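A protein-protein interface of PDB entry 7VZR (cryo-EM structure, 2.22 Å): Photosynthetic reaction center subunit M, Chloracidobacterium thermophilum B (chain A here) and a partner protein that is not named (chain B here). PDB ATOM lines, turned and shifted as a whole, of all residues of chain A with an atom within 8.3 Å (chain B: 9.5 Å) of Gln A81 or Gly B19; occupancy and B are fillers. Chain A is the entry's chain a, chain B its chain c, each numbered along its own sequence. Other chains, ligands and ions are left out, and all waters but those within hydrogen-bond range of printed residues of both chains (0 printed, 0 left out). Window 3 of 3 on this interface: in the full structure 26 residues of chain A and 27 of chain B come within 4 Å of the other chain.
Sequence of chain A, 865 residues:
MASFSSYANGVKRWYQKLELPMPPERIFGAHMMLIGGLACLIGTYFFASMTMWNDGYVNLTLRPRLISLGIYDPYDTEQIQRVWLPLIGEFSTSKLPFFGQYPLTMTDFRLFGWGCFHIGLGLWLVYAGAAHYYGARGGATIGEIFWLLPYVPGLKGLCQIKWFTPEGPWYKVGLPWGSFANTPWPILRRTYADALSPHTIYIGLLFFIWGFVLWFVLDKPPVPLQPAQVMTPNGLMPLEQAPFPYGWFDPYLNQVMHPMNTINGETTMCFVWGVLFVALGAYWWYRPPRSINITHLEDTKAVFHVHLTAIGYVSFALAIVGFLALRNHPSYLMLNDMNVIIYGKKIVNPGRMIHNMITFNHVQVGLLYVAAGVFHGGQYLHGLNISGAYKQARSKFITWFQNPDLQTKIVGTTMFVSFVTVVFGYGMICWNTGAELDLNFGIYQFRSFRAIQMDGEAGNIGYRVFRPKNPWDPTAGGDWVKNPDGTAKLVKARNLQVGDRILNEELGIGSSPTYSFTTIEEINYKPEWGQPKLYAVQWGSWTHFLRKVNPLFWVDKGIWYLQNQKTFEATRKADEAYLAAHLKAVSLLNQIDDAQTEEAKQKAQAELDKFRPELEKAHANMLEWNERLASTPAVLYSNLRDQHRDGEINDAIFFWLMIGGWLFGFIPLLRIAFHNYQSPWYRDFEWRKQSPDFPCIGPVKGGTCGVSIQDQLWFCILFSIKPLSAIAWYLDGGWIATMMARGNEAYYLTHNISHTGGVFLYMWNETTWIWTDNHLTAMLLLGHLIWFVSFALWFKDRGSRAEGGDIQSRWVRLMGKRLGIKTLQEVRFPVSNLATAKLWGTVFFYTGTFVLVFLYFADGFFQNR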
ATOM      1  N   THR A  77     -19.483 -21.553  35.633  1.00  0.00           N
ATOM      2  CA  THR A  77     -20.888 -21.556  35.941  1.00  0.00           C
ATOM      3  C   THR A  77     -21.753 -21.138  34.776  1.00  0.00           C
ATOM      4  O   THR A  77     -22.942 -21.370  34.823  1.00  0.00           O
ATOM      5  CB  THR A  77     -21.182 -20.636  37.134  1.00  0.00           C
ATOM      6  OG1 THR A  77     -20.819 -19.310  36.794  1.00  0.00           O
ATOM      7  CG2 THR A  77     -20.417 -21.048  38.346  1.00  0.00           C
ATOM      8  N   GLU A  78     -21.187 -20.617  33.717  1.00  0.00           N
ATOM      9  CA  GLU A  78     -21.997 -20.033  32.669  1.00  0.00           C
ATOM     10  C   GLU A  78     -22.805 -21.096  31.951  1.00  0.00           C
ATOM     11  O   GLU A  78     -22.281 -22.131  31.557  1.00  0.00           O
ATOM     12  CB  GLU A  78     -21.128 -19.280  31.683  1.00  0.00           C
ATOM     13  CG  GLU A  78     -21.976 -18.702  30.633  1.00  0.00           C
ATOM     14  CD  GLU A  78     -21.232 -18.087  29.470  1.00  0.00           C
ATOM     15  OE1 GLU A  78     -20.578 -17.039  29.646  1.00  0.00           O
ATOM     16  OE2 GLU A  78     -21.316 -18.637  28.349  1.00  0.00           O
ATOM     17  N   GLN A  79     -24.097 -20.899  31.805  1.00  0.00           N
ATOM     18  CA  GLN A  79     -24.936 -21.870  31.160  1.00  0.00           C
ATOM     19  C   GLN A  79     -24.901 -21.683  29.672  1.00  0.00           C
ATOM     20  O   GLN A  79     -24.714 -20.667  29.223  1.00  0.00           O
ATOM     21  CB  GLN A  79     -26.342 -21.914  31.805  1.00  0.00           C
ATOM     22  CG  GLN A  79     -27.502 -21.564  30.961  1.00  0.00           C
ATOM     23  CD  GLN A  79     -28.638 -22.546  31.023  1.00  0.00           C
ATOM     24  OE1 GLN A  79     -28.854 -23.153  31.998  1.00  0.00           O
ATOM     25  NE2 GLN A  79     -29.374 -22.684  29.946  1.00  0.00           N
ATOM     26  N   ILE A  80     -24.949 -22.742  28.929  1.00  0.00           N
ATOM     27  CA  ILE A  80     -24.866 -22.786  27.474  1.00  0.00           C
ATOM     28  C   ILE A  80     -26.250 -23.056  26.930  1.00  0.00           C
ATOM     29  O   ILE A  80     -27.008 -23.802  27.542  1.00  0.00           O
ATOM     30  CB  ILE A  80     -23.912 -23.892  27.014  1.00  0.00           C
ATOM     31  CG1 ILE A  80     -22.598 -23.832  27.743  1.00  0.00           C
ATOM     32  CG2 ILE A  80     -23.679 -23.773  25.583  1.00  0.00           C
ATOM     33  CD1 ILE A  80     -21.580 -23.158  27.074  1.00  0.00           C
ATOM     34  N   GLN A  81     -26.558 -22.361  25.830  1.00  0.00           N
ATOM     35  CA  GLN A  81     -27.826 -22.402  25.164  1.00  0.00           C
ATOM     36  C   GLN A  81     -27.865 -22.616  23.661  1.00  0.00           C
ATOM     37  O   GLN A  81     -28.943 -22.500  23.109  1.00  0.00           O
ATOM     38  CB  GLN A  81     -28.531 -21.100  25.430  1.00  0.00           C
ATOM     39  CG  GLN A  81     -29.057 -21.008  26.829  1.00  0.00           C
ATOM     40  CD  GLN A  81     -28.589 -19.768  27.535  1.00  0.00           C
ATOM     41  OE1 GLN A  81     -28.911 -19.537  28.684  1.00  0.00           O
ATOM     42  NE2 GLN A  81     -27.816 -18.969  26.850  1.00  0.00           N
ATOM     43  N   ARG A  82     -26.751 -22.922  22.999  1.00  0.00           N
ATOM     44  CA  ARG A  82     -26.776 -23.147  21.544  1.00  0.00           C
ATOM     45  C   ARG A  82     -25.635 -23.965  20.915  1.00  0.00           C
ATOM     46  O   ARG A  82     -25.876 -24.741  20.004  1.00  0.00           O
ATOM     47  CB  ARG A  82     -26.849 -21.826  20.793  1.00  0.00           C
ATOM     48  CG  ARG A  82     -26.251 -21.895  19.405  1.00  0.00           C
ATOM     49  CD  ARG A  82     -25.257 -20.764  19.161  1.00  0.00           C
ATOM     50  NE  ARG A  82     -23.885 -21.239  19.151  1.00  0.00           N
ATOM     51  CZ  ARG A  82     -23.035 -21.047  20.144  1.00  0.00           C
ATOM     52  NH1 ARG A  82     -23.423 -20.397  21.208  1.00  0.00           N
ATOM     53  NH2 ARG A  82     -21.807 -21.505  20.064  1.00  0.00           N
ATOM     54  N   VAL A  83     -24.405 -23.744  21.406  1.00  0.00           N
ATOM     55  CA  VAL A  83     -23.096 -24.337  20.988  1.00  0.00           C
ATOM     56  C   VAL A  83     -22.775 -24.693  19.569  1.00  0.00           C
ATOM     57  O   VAL A  83     -21.928 -24.057  18.969  1.00  0.00           O
ATOM     58  CB  VAL A  83     -22.615 -25.546  21.782  1.00  0.00           C
ATOM     59  CG1 VAL A  83     -21.682 -25.120  22.891  1.00  0.00           C
ATOM     60  CG2 VAL A  83     -23.750 -26.464  22.209  1.00  0.00           C
ATOM     61  N   TRP A  84     -23.376 -25.760  19.065  1.00  0.00           N
ATOM     62  CA  TRP A  84     -23.123 -26.203  17.697  1.00  0.00           C
ATOM     63  C   TRP A  84     -24.287 -25.906  16.732  1.00  0.00           C
ATOM     64  O   TRP A  84     -24.521 -24.761  16.356  1.00  0.00           O
ATOM     65  CB  TRP A  84     -22.785 -27.689  17.698  1.00  0.00           C
ATOM     66  CG  TRP A  84     -21.463 -27.978  17.080  1.00  0.00           C
ATOM     67  CD1 TRP A  84     -20.435 -27.118  16.935  1.00  0.00           C
ATOM     68  CD2 TRP A  84     -21.037 -29.220  16.519  1.00  0.00           C
ATOM     69  NE1 TRP A  84     -19.387 -27.739  16.323  1.00  0.00           N
ATOM     70  CE2 TRP A  84     -19.731 -29.037  16.059  1.00  0.00           C
ATOM     71  CE3 TRP A  84     -21.635 -30.472  16.367  1.00  0.00           C
ATOM     72  CZ2 TRP A  84     -19.003 -30.060  15.453  1.00  0.00           C
ATOM     73  CZ3 TRP A  84     -20.923 -31.481  15.766  1.00  0.00           C
ATOM     74  CH2 TRP A  84     -19.615 -31.274  15.318  1.00  0.00           C
ATOM     75  N   LEU A  85     -25.035 -26.934  16.348  1.00  0.00           N
ATOM     76  CA  LEU A  85     -26.147 -26.731  15.446  1.00  0.00           C
ATOM     77  C   LEU A  85     -27.150 -25.758  16.028  1.00  0.00           C
ATOM     78  O   LEU A  85     -27.453 -25.799  17.202  1.00  0.00           O
ATOM     79  CB  LEU A  85     -26.812 -28.061  15.085  1.00  0.00           C
ATOM     80  CG  LEU A  85     -27.376 -29.005  16.149  1.00  0.00           C
ATOM     81  CD1 LEU A  85     -27.636 -30.384  15.570  1.00  0.00           C
ATOM     82  CD2 LEU A  85     -26.395 -29.102  17.298  1.00  0.00           C
ATOM     83  N   PRO A  86     -27.658 -24.863  15.176  1.00  0.00           N
ATOM     84  CA  PRO A  86     -28.628 -23.764  15.331  1.00  0.00           C
ATOM     85  C   PRO A  86     -29.816 -24.007  16.253  1.00  0.00           C
ATOM     86  O   PRO A  86     -30.397 -25.062  16.148  1.00  0.00           O
ATOM     87  CB  PRO A  86     -29.177 -23.586  13.908  1.00  0.00           C
ATOM     88  CG  PRO A  86     -28.281 -24.379  13.009  1.00  0.00           C
ATOM     89  CD  PRO A  86     -27.125 -24.897  13.813  1.00  0.00           C
ATOM     90  N   LEU A  87     -30.164 -23.042  17.105  1.00  0.00           N
ATOM     91  CA  LEU A  87     -31.329 -23.120  18.002  1.00  0.00           C
ATOM     92  C   LEU A  87     -31.545 -24.331  18.936  1.00  0.00           C
ATOM     93  O   LEU A  87     -32.231 -25.263  18.549  1.00  0.00           O
ATOM     94  CB  LEU A  87     -32.606 -22.964  17.177  1.00  0.00           C
ATOM     95  CG  LEU A  87     -32.673 -22.230  15.830  1.00  0.00           C
ATOM     96  CD1 LEU A  87     -33.167 -23.179  14.747  1.00  0.00           C
ATOM     97  CD2 LEU A  87     -33.581 -21.005  15.910  1.00  0.00           C
ATOM     98  N   ILE A  88     -31.068 -24.290  20.183  1.00  0.00           N
ATOM     99  CA  ILE A  88     -31.252 -25.452  21.059  1.00  0.00           C
ATOM    100  C   ILE A  88     -31.652 -25.349  22.573  1.00  0.00           C
ATOM    101  O   ILE A  88     -31.010 -25.943  23.448  1.00  0.00           O
ATOM    102  CB  ILE A  88     -30.175 -26.563  20.839  1.00  0.00           C
ATOM    103  CG1 ILE A  88     -28.899 -26.069  20.177  1.00  0.00           C
ATOM    104  CG2 ILE A  88     -30.706 -27.696  19.969  1.00  0.00           C
ATOM    105  CD1 ILE A  88     -27.923 -27.207  20.045  1.00  0.00           C
ATOM    106  N   GLY A  89     -32.694 -24.572  22.854  1.00  0.00           N
ATOM    107  CA  GLY A  89     -33.352 -24.528  24.152  1.00  0.00           C
ATOM    108  C   GLY A  89     -33.509 -25.913  24.774  1.00  0.00           C
ATOM    109  O   GLY A  89     -32.991 -26.181  25.865  1.00  0.00           O
ATOM    110  N   GLU A  90     -34.224 -26.802  24.083  1.00  0.00           N
ATOM    111  CA  GLU A  90     -34.259 -28.226  24.359  1.00  0.00           C
ATOM    112  C   GLU A  90     -35.114 -28.899  23.293  1.00  0.00           C
ATOM    113  O   GLU A  90     -36.024 -28.272  22.751  1.00  0.00           O
ATOM    114  CB  GLU A  90     -34.812 -28.483  25.756  1.00  0.00           C
ATOM    115  CG  GLU A  90     -36.180 -27.914  25.962  1.00  0.00           C
ATOM    116  CD  GLU A  90     -36.176 -26.521  26.566  1.00  0.00           C
ATOM    117  OE1 GLU A  90     -35.987 -26.408  27.788  1.00  0.00           O
ATOM    118  OE2 GLU A  90     -36.377 -25.549  25.817  1.00  0.00           O
ATOM    119  N   LYS A  95     -31.786 -31.676  23.007  1.00  0.00           N
ATOM    120  CA  LYS A  95     -30.541 -30.962  22.680  1.00  0.00           C
ATOM    121  C   LYS A  95     -29.331 -31.818  23.037  1.00  0.00           C
ATOM    122  O   LYS A  95     -28.290 -31.771  22.372  1.00  0.00           O
ATOM    123  CB  LYS A  95     -30.510 -29.613  23.403  1.00  0.00           C
ATOM    124  CG  LYS A  95     -29.230 -29.236  24.135  1.00  0.00           C
ATOM    125  CD  LYS A  95     -29.419 -27.889  24.803  1.00  0.00           C
ATOM    126  CE  LYS A  95     -28.175 -26.972  24.789  1.00  0.00           C
ATOM    127  NZ  LYS A  95     -28.243 -25.997  25.868  1.00  0.00           N
ATOM    128  N   PRO A 103     -29.796 -27.464  33.091  1.00  0.00           N
ATOM    129  CA  PRO A 103     -28.873 -26.416  32.632  1.00  0.00           C
ATOM    130  C   PRO A 103     -27.463 -26.966  32.500  1.00  0.00           C
ATOM    131  O   PRO A 103     -27.008 -27.723  33.334  1.00  0.00           O
ATOM    132  CB  PRO A 103     -28.968 -25.360  33.731  1.00  0.00           C
ATOM    133  CG  PRO A 103     -29.360 -26.087  34.932  1.00  0.00           C
ATOM    134  CD  PRO A 103     -30.128 -27.321  34.513  1.00  0.00           C
ATOM    135  N   LEU A 104     -26.812 -26.666  31.402  1.00  0.00           N
ATOM    136  CA  LEU A 104     -25.509 -27.255  31.137  1.00  0.00           C
ATOM    137  C   LEU A 104     -24.429 -26.211  30.932  1.00  0.00           C
ATOM    138  O   LEU A 104     -24.645 -25.209  30.265  1.00  0.00           O
ATOM    139  CB  LEU A 104     -25.547 -28.128  29.915  1.00  0.00           C
ATOM    140  CG  LEU A 104     -26.599 -29.213  29.857  1.00  0.00           C
ATOM    141  CD1 LEU A 104     -26.593 -29.738  28.510  1.00  0.00           C
ATOM    142  CD2 LEU A 104     -26.274 -30.317  30.755  1.00  0.00           C
ATOM    143  N   THR A 105     -23.259 -26.492  31.447  1.00  0.00           N
ATOM    144  CA  THR A 105     -22.052 -25.718  31.248  1.00  0.00           C
ATOM    145  C   THR A 105     -21.140 -26.383  30.228  1.00  0.00           C
ATOM    146  O   THR A 105     -21.387 -27.466  29.747  1.00  0.00           O
ATOM    147  CB  THR A 105     -21.330 -25.479  32.582  1.00  0.00           C
ATOM    148  OG1 THR A 105     -20.850 -26.696  33.147  1.00  0.00           O
ATOM    149  CG2 THR A 105     -22.225 -24.833  33.597  1.00  0.00           C
ATOM    150  N   PHE A 109     -20.469 -30.439  28.489  1.00  0.00           N
ATOM    151  CA  PHE A 109     -20.296 -30.818  27.111  1.00  0.00           C
ATOM    152  C   PHE A 109     -19.007 -31.561  26.903  1.00  0.00           C
ATOM    153  O   PHE A 109     -18.948 -32.454  26.067  1.00  0.00           O
ATOM    154  CB  PHE A 109     -20.301 -29.622  26.193  1.00  0.00           C
ATOM    155  CG  PHE A 109     -21.614 -29.210  25.811  1.00  0.00           C
ATOM    156  CD1 PHE A 109     -22.240 -29.779  24.743  1.00  0.00           C
ATOM    157  CD2 PHE A 109     -22.283 -28.259  26.552  1.00  0.00           C
ATOM    158  CE1 PHE A 109     -23.515 -29.374  24.381  1.00  0.00           C
ATOM    159  CE2 PHE A 109     -23.561 -27.838  26.222  1.00  0.00           C
ATOM    160  CZ  PHE A 109     -24.178 -28.383  25.140  1.00  0.00           C
ATOM    161  N   GLU B  15     -31.753 -20.819  44.048  1.00  0.00           N
ATOM    162  CA  GLU B  15     -32.575 -20.233  43.024  1.00  0.00           C
ATOM    163  C   GLU B  15     -31.922 -20.017  41.705  1.00  0.00           C
ATOM    164  O   GLU B  15     -30.767 -19.616  41.640  1.00  0.00           O
ATOM    165  CB  GLU B  15     -33.048 -18.866  43.461  1.00  0.00           C
ATOM    166  CG  GLU B  15     -32.654 -18.489  44.883  1.00  0.00           C
ATOM    167  CD  GLU B  15     -33.656 -17.546  45.529  1.00  0.00           C
ATOM    168  OE1 GLU B  15     -33.659 -16.344  45.155  1.00  0.00           O
ATOM    169  OE2 GLU B  15     -34.419 -18.014  46.458  1.00  0.00           O
ATOM    170  N   PRO B  16     -32.704 -20.187  40.652  1.00  0.00           N
ATOM    171  CA  PRO B  16     -32.074 -19.907  39.374  1.00  0.00           C
ATOM    172  C   PRO B  16     -32.189 -18.496  38.857  1.00  0.00           C
ATOM    173  O   PRO B  16     -33.255 -17.847  38.864  1.00  0.00           O
ATOM    174  CB  PRO B  16     -32.710 -20.880  38.423  1.00  0.00           C
ATOM    175  CG  PRO B  16     -33.945 -21.357  39.095  1.00  0.00           C
ATOM    176  CD  PRO B  16     -33.787 -21.161  40.570  1.00  0.00           C
ATOM    177  N   ARG B  17     -31.049 -18.063  38.377  1.00  0.00           N
ATOM    178  CA  ARG B  17     -30.853 -16.809  37.761  1.00  0.00           C
ATOM    179  C   ARG B  17     -30.616 -17.194  36.357  1.00  0.00           C
ATOM    180  O   ARG B  17     -29.845 -18.064  36.052  1.00  0.00           O
ATOM    181  CB  ARG B  17     -29.618 -16.141  38.265  1.00  0.00           C
ATOM    182  CG  ARG B  17     -29.415 -14.811  37.573  1.00  0.00           C
ATOM    183  CD  ARG B  17     -28.107 -14.150  37.898  1.00  0.00           C
ATOM    184  NE  ARG B  17     -27.418 -14.872  38.947  1.00  0.00           N
ATOM    185  CZ  ARG B  17     -26.151 -15.224  38.892  1.00  0.00           C
ATOM    186  NH1 ARG B  17     -25.668 -15.903  39.897  1.00  0.00           N
ATOM    187  NH2 ARG B  17     -25.385 -14.891  37.860  1.00  0.00           N
ATOM    188  N   LEU B  18     -31.285 -16.548  35.473  1.00  0.00           N
ATOM    189  CA  LEU B  18     -31.142 -16.882  34.090  1.00  0.00           C
ATOM    190  C   LEU B  18     -29.778 -16.735  33.460  1.00  0.00           C
ATOM    191  O   LEU B  18     -29.104 -15.762  33.623  1.00  0.00           O
ATOM    192  CB  LEU B  18     -32.281 -16.254  33.271  1.00  0.00           C
ATOM    193  CG  LEU B  18     -31.956 -15.641  31.935  1.00  0.00           C
ATOM    194  CD1 LEU B  18     -33.255 -15.082  31.375  1.00  0.00           C
ATOM    195  CD2 LEU B  18     -31.005 -14.508  32.171  1.00  0.00           C
ATOM    196  N   GLY B  19     -29.362 -17.823  32.817  1.00  0.00           N
ATOM    197  CA  GLY B  19     -28.120 -17.866  32.082  1.00  0.00           C
ATOM    198  C   GLY B  19     -26.913 -18.269  32.877  1.00  0.00           C
ATOM    199  O   GLY B  19     -25.805 -18.000  32.464  1.00  0.00           O
ATOM    200  N   SER B  20     -27.097 -18.866  34.033  1.00  0.00           N
ATOM    201  CA  SER B  20     -25.969 -19.169  34.888  1.00  0.00           C
ATOM    202  C   SER B  20     -26.345 -20.297  35.818  1.00  0.00           C
ATOM    203  O   SER B  20     -26.984 -20.042  36.831  1.00  0.00           O
ATOM    204  CB  SER B  20     -25.595 -17.956  35.674  1.00  0.00           C
ATOM    205  OG  SER B  20     -24.935 -18.372  36.826  1.00  0.00           O
ATOM    206  N   SER B  21     -25.966 -21.500  35.491  1.00  0.00           N
ATOM    207  CA  SER B  21     -26.320 -22.692  36.218  1.00  0.00           C
ATOM    208  C   SER B  21     -26.283 -22.605  37.771  1.00  0.00           C
ATOM    209  O   SER B  21     -25.318 -22.273  38.297  1.00  0.00           O
ATOM    210  CB  SER B  21     -25.444 -23.754  35.638  1.00  0.00           C
ATOM    211  OG  SER B  21     -25.589 -24.983  36.177  1.00  0.00           O
ATOM    212  N   SER B  22     -27.371 -22.848  38.459  1.00  0.00           N
ATOM    213  CA  SER B  22     -27.392 -22.797  39.869  1.00  0.00           C
ATOM    214  C   SER B  22     -26.800 -24.010  40.507  1.00  0.00           C
ATOM    215  O   SER B  22     -26.269 -23.898  41.514  1.00  0.00           O
ATOM    216  CB  SER B  22     -28.754 -22.527  40.409  1.00  0.00           C
ATOM    217  OG  SER B  22     -29.578 -23.573  40.040  1.00  0.00           O
ATOM    218  N   ALA B  24     -24.324 -25.662  39.227  1.00  0.00           N
ATOM    219  CA  ALA B  24     -22.922 -25.469  39.127  1.00  0.00           C
ATOM    220  C   ALA B  24     -22.479 -24.545  40.147  1.00  0.00           C
ATOM    221  O   ALA B  24     -21.617 -24.887  40.821  1.00  0.00           O
ATOM    222  CB  ALA B  24     -22.475 -25.019  37.781  1.00  0.00           C
ATOM    223  N   ASP B  54     -27.251  -8.167  36.242  1.00  0.00           N
ATOM    224  CA  ASP B  54     -28.235  -9.216  36.497  1.00  0.00           C
ATOM    225  C   ASP B  54     -28.040  -9.855  37.870  1.00  0.00           C
ATOM    226  O   ASP B  54     -29.013 -10.198  38.546  1.00  0.00           O
ATOM    227  CB  ASP B  54     -28.183 -10.283  35.403  1.00  0.00           C
ATOM    228  CG  ASP B  54     -26.772 -10.759  35.113  1.00  0.00           C
ATOM    229  OD1 ASP B  54     -25.912  -9.912  34.792  1.00  0.00           O
ATOM    230  OD2 ASP B  54     -26.522 -11.979  35.208  1.00  0.00           O
ATOM    231  N   GLU B  55     -26.786 -10.008  38.279  1.00  0.00           N
ATOM    232  CA  GLU B  55     -26.470 -10.602  39.568  1.00  0.00           C
ATOM    233  C   GLU B  55     -26.915  -9.696  40.714  1.00  0.00           C
ATOM    234  O   GLU B  55     -27.573 -10.143  41.651  1.00  0.00           O
ATOM    235  CB  GLU B  55     -24.970 -10.888  39.677  1.00  0.00           C
ATOM    236  CG  GLU B  55     -24.634 -12.183  40.397  1.00  0.00           C
ATOM    237  CD  GLU B  55     -23.230 -12.670  40.098  1.00  0.00           C
ATOM    238  OE1 GLU B  55     -22.847 -12.692  38.909  1.00  0.00           O
ATOM    239  OE2 GLU B  55     -22.507 -13.028  41.052  1.00  0.00           O
ATOM    240  N   HIS B  58     -30.803  -9.844  41.140  1.00  0.00           N
ATOM    241  CA  HIS B  58     -31.325 -11.090  41.504  1.00  0.00           C
ATOM    242  C   HIS B  58     -31.175 -11.211  43.014  1.00  0.00           C
ATOM    243  O   HIS B  58     -31.967 -11.749  43.649  1.00  0.00           O
ATOM    244  CB  HIS B  58     -30.519 -12.121  40.800  1.00  0.00           C
ATOM    245  CG  HIS B  58     -30.705 -13.505  41.298  1.00  0.00           C
ATOM    246  ND1 HIS B  58     -31.704 -14.318  40.837  1.00  0.00           N
ATOM    247  CD2 HIS B  58     -30.021 -14.223  42.200  1.00  0.00           C
ATOM    248  CE1 HIS B  58     -31.626 -15.481  41.450  1.00  0.00           C
ATOM    249  NE2 HIS B  58     -30.620 -15.442  42.285  1.00  0.00           N
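Ser B20 touches Thr A77 (C to O, 3.7 Å).
Gln A79 touches Ser B20.
Gln A79 touches Ser B21 (CB to N, 3.7 Å).
Gly B19 touches Gln A81.
Thr A105 touches Ser B21 (CG2 to CB, 3.96 Å).
The backbone NH (N) of Ser B21 is in hydrogen-bond range of the backbone carbonyl oxygen (O) of Thr A77 (3.1 Å).
O of Gly B19 is in hydrogen-bond range of N of Gln A79, 3.4 Å away.
The side-chain hydroxyl (OG) of Ser B21 lies within hydrogen-bond range of the backbone NH (N) of Ala B24 (3.4 Å).
The side-chain amide oxygen (OE1) of Gln A81 sits close to the side-chain amide nitrogen (NE2) of Gln A79 (3.4 Å).
Of the 12 printed residues of chain B, 3 touch a printed residue of chain A.
Of the 19 printed residues of chain A, 4 touch a printed residue of chain B.
Along chain A the printed residues that touch a printed residue of chain B span positions 77 to 105.
Among the printed residues, 7 pairs touch across the chains.
Printed residues of chain B within 4 Å of Thr A77: Ser B20 (3.7 Å) and Ser B21 (3.1 Å).
Of the printed residues of chain B, Gln A79 touches Gly B19, Ser B20 and Ser B21.
No residue of chain B comes within 4 Å of Ile A80.
Of chain B, only Gly B19 (3.9 Å) comes within 4 Å of Gln A81.
Leu A104 touches none of the printed residues of chain B.
Of the printed residues of chain A, Ser B20 touches Thr A77 and Gln A79.
Of the printed residues of chain A, Ser B21 touches Thr A77, Gln A79 and Thr A105.
The nearest residue of chain A that does not touch Gly B19 is Glu A78 (4.3 Å).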
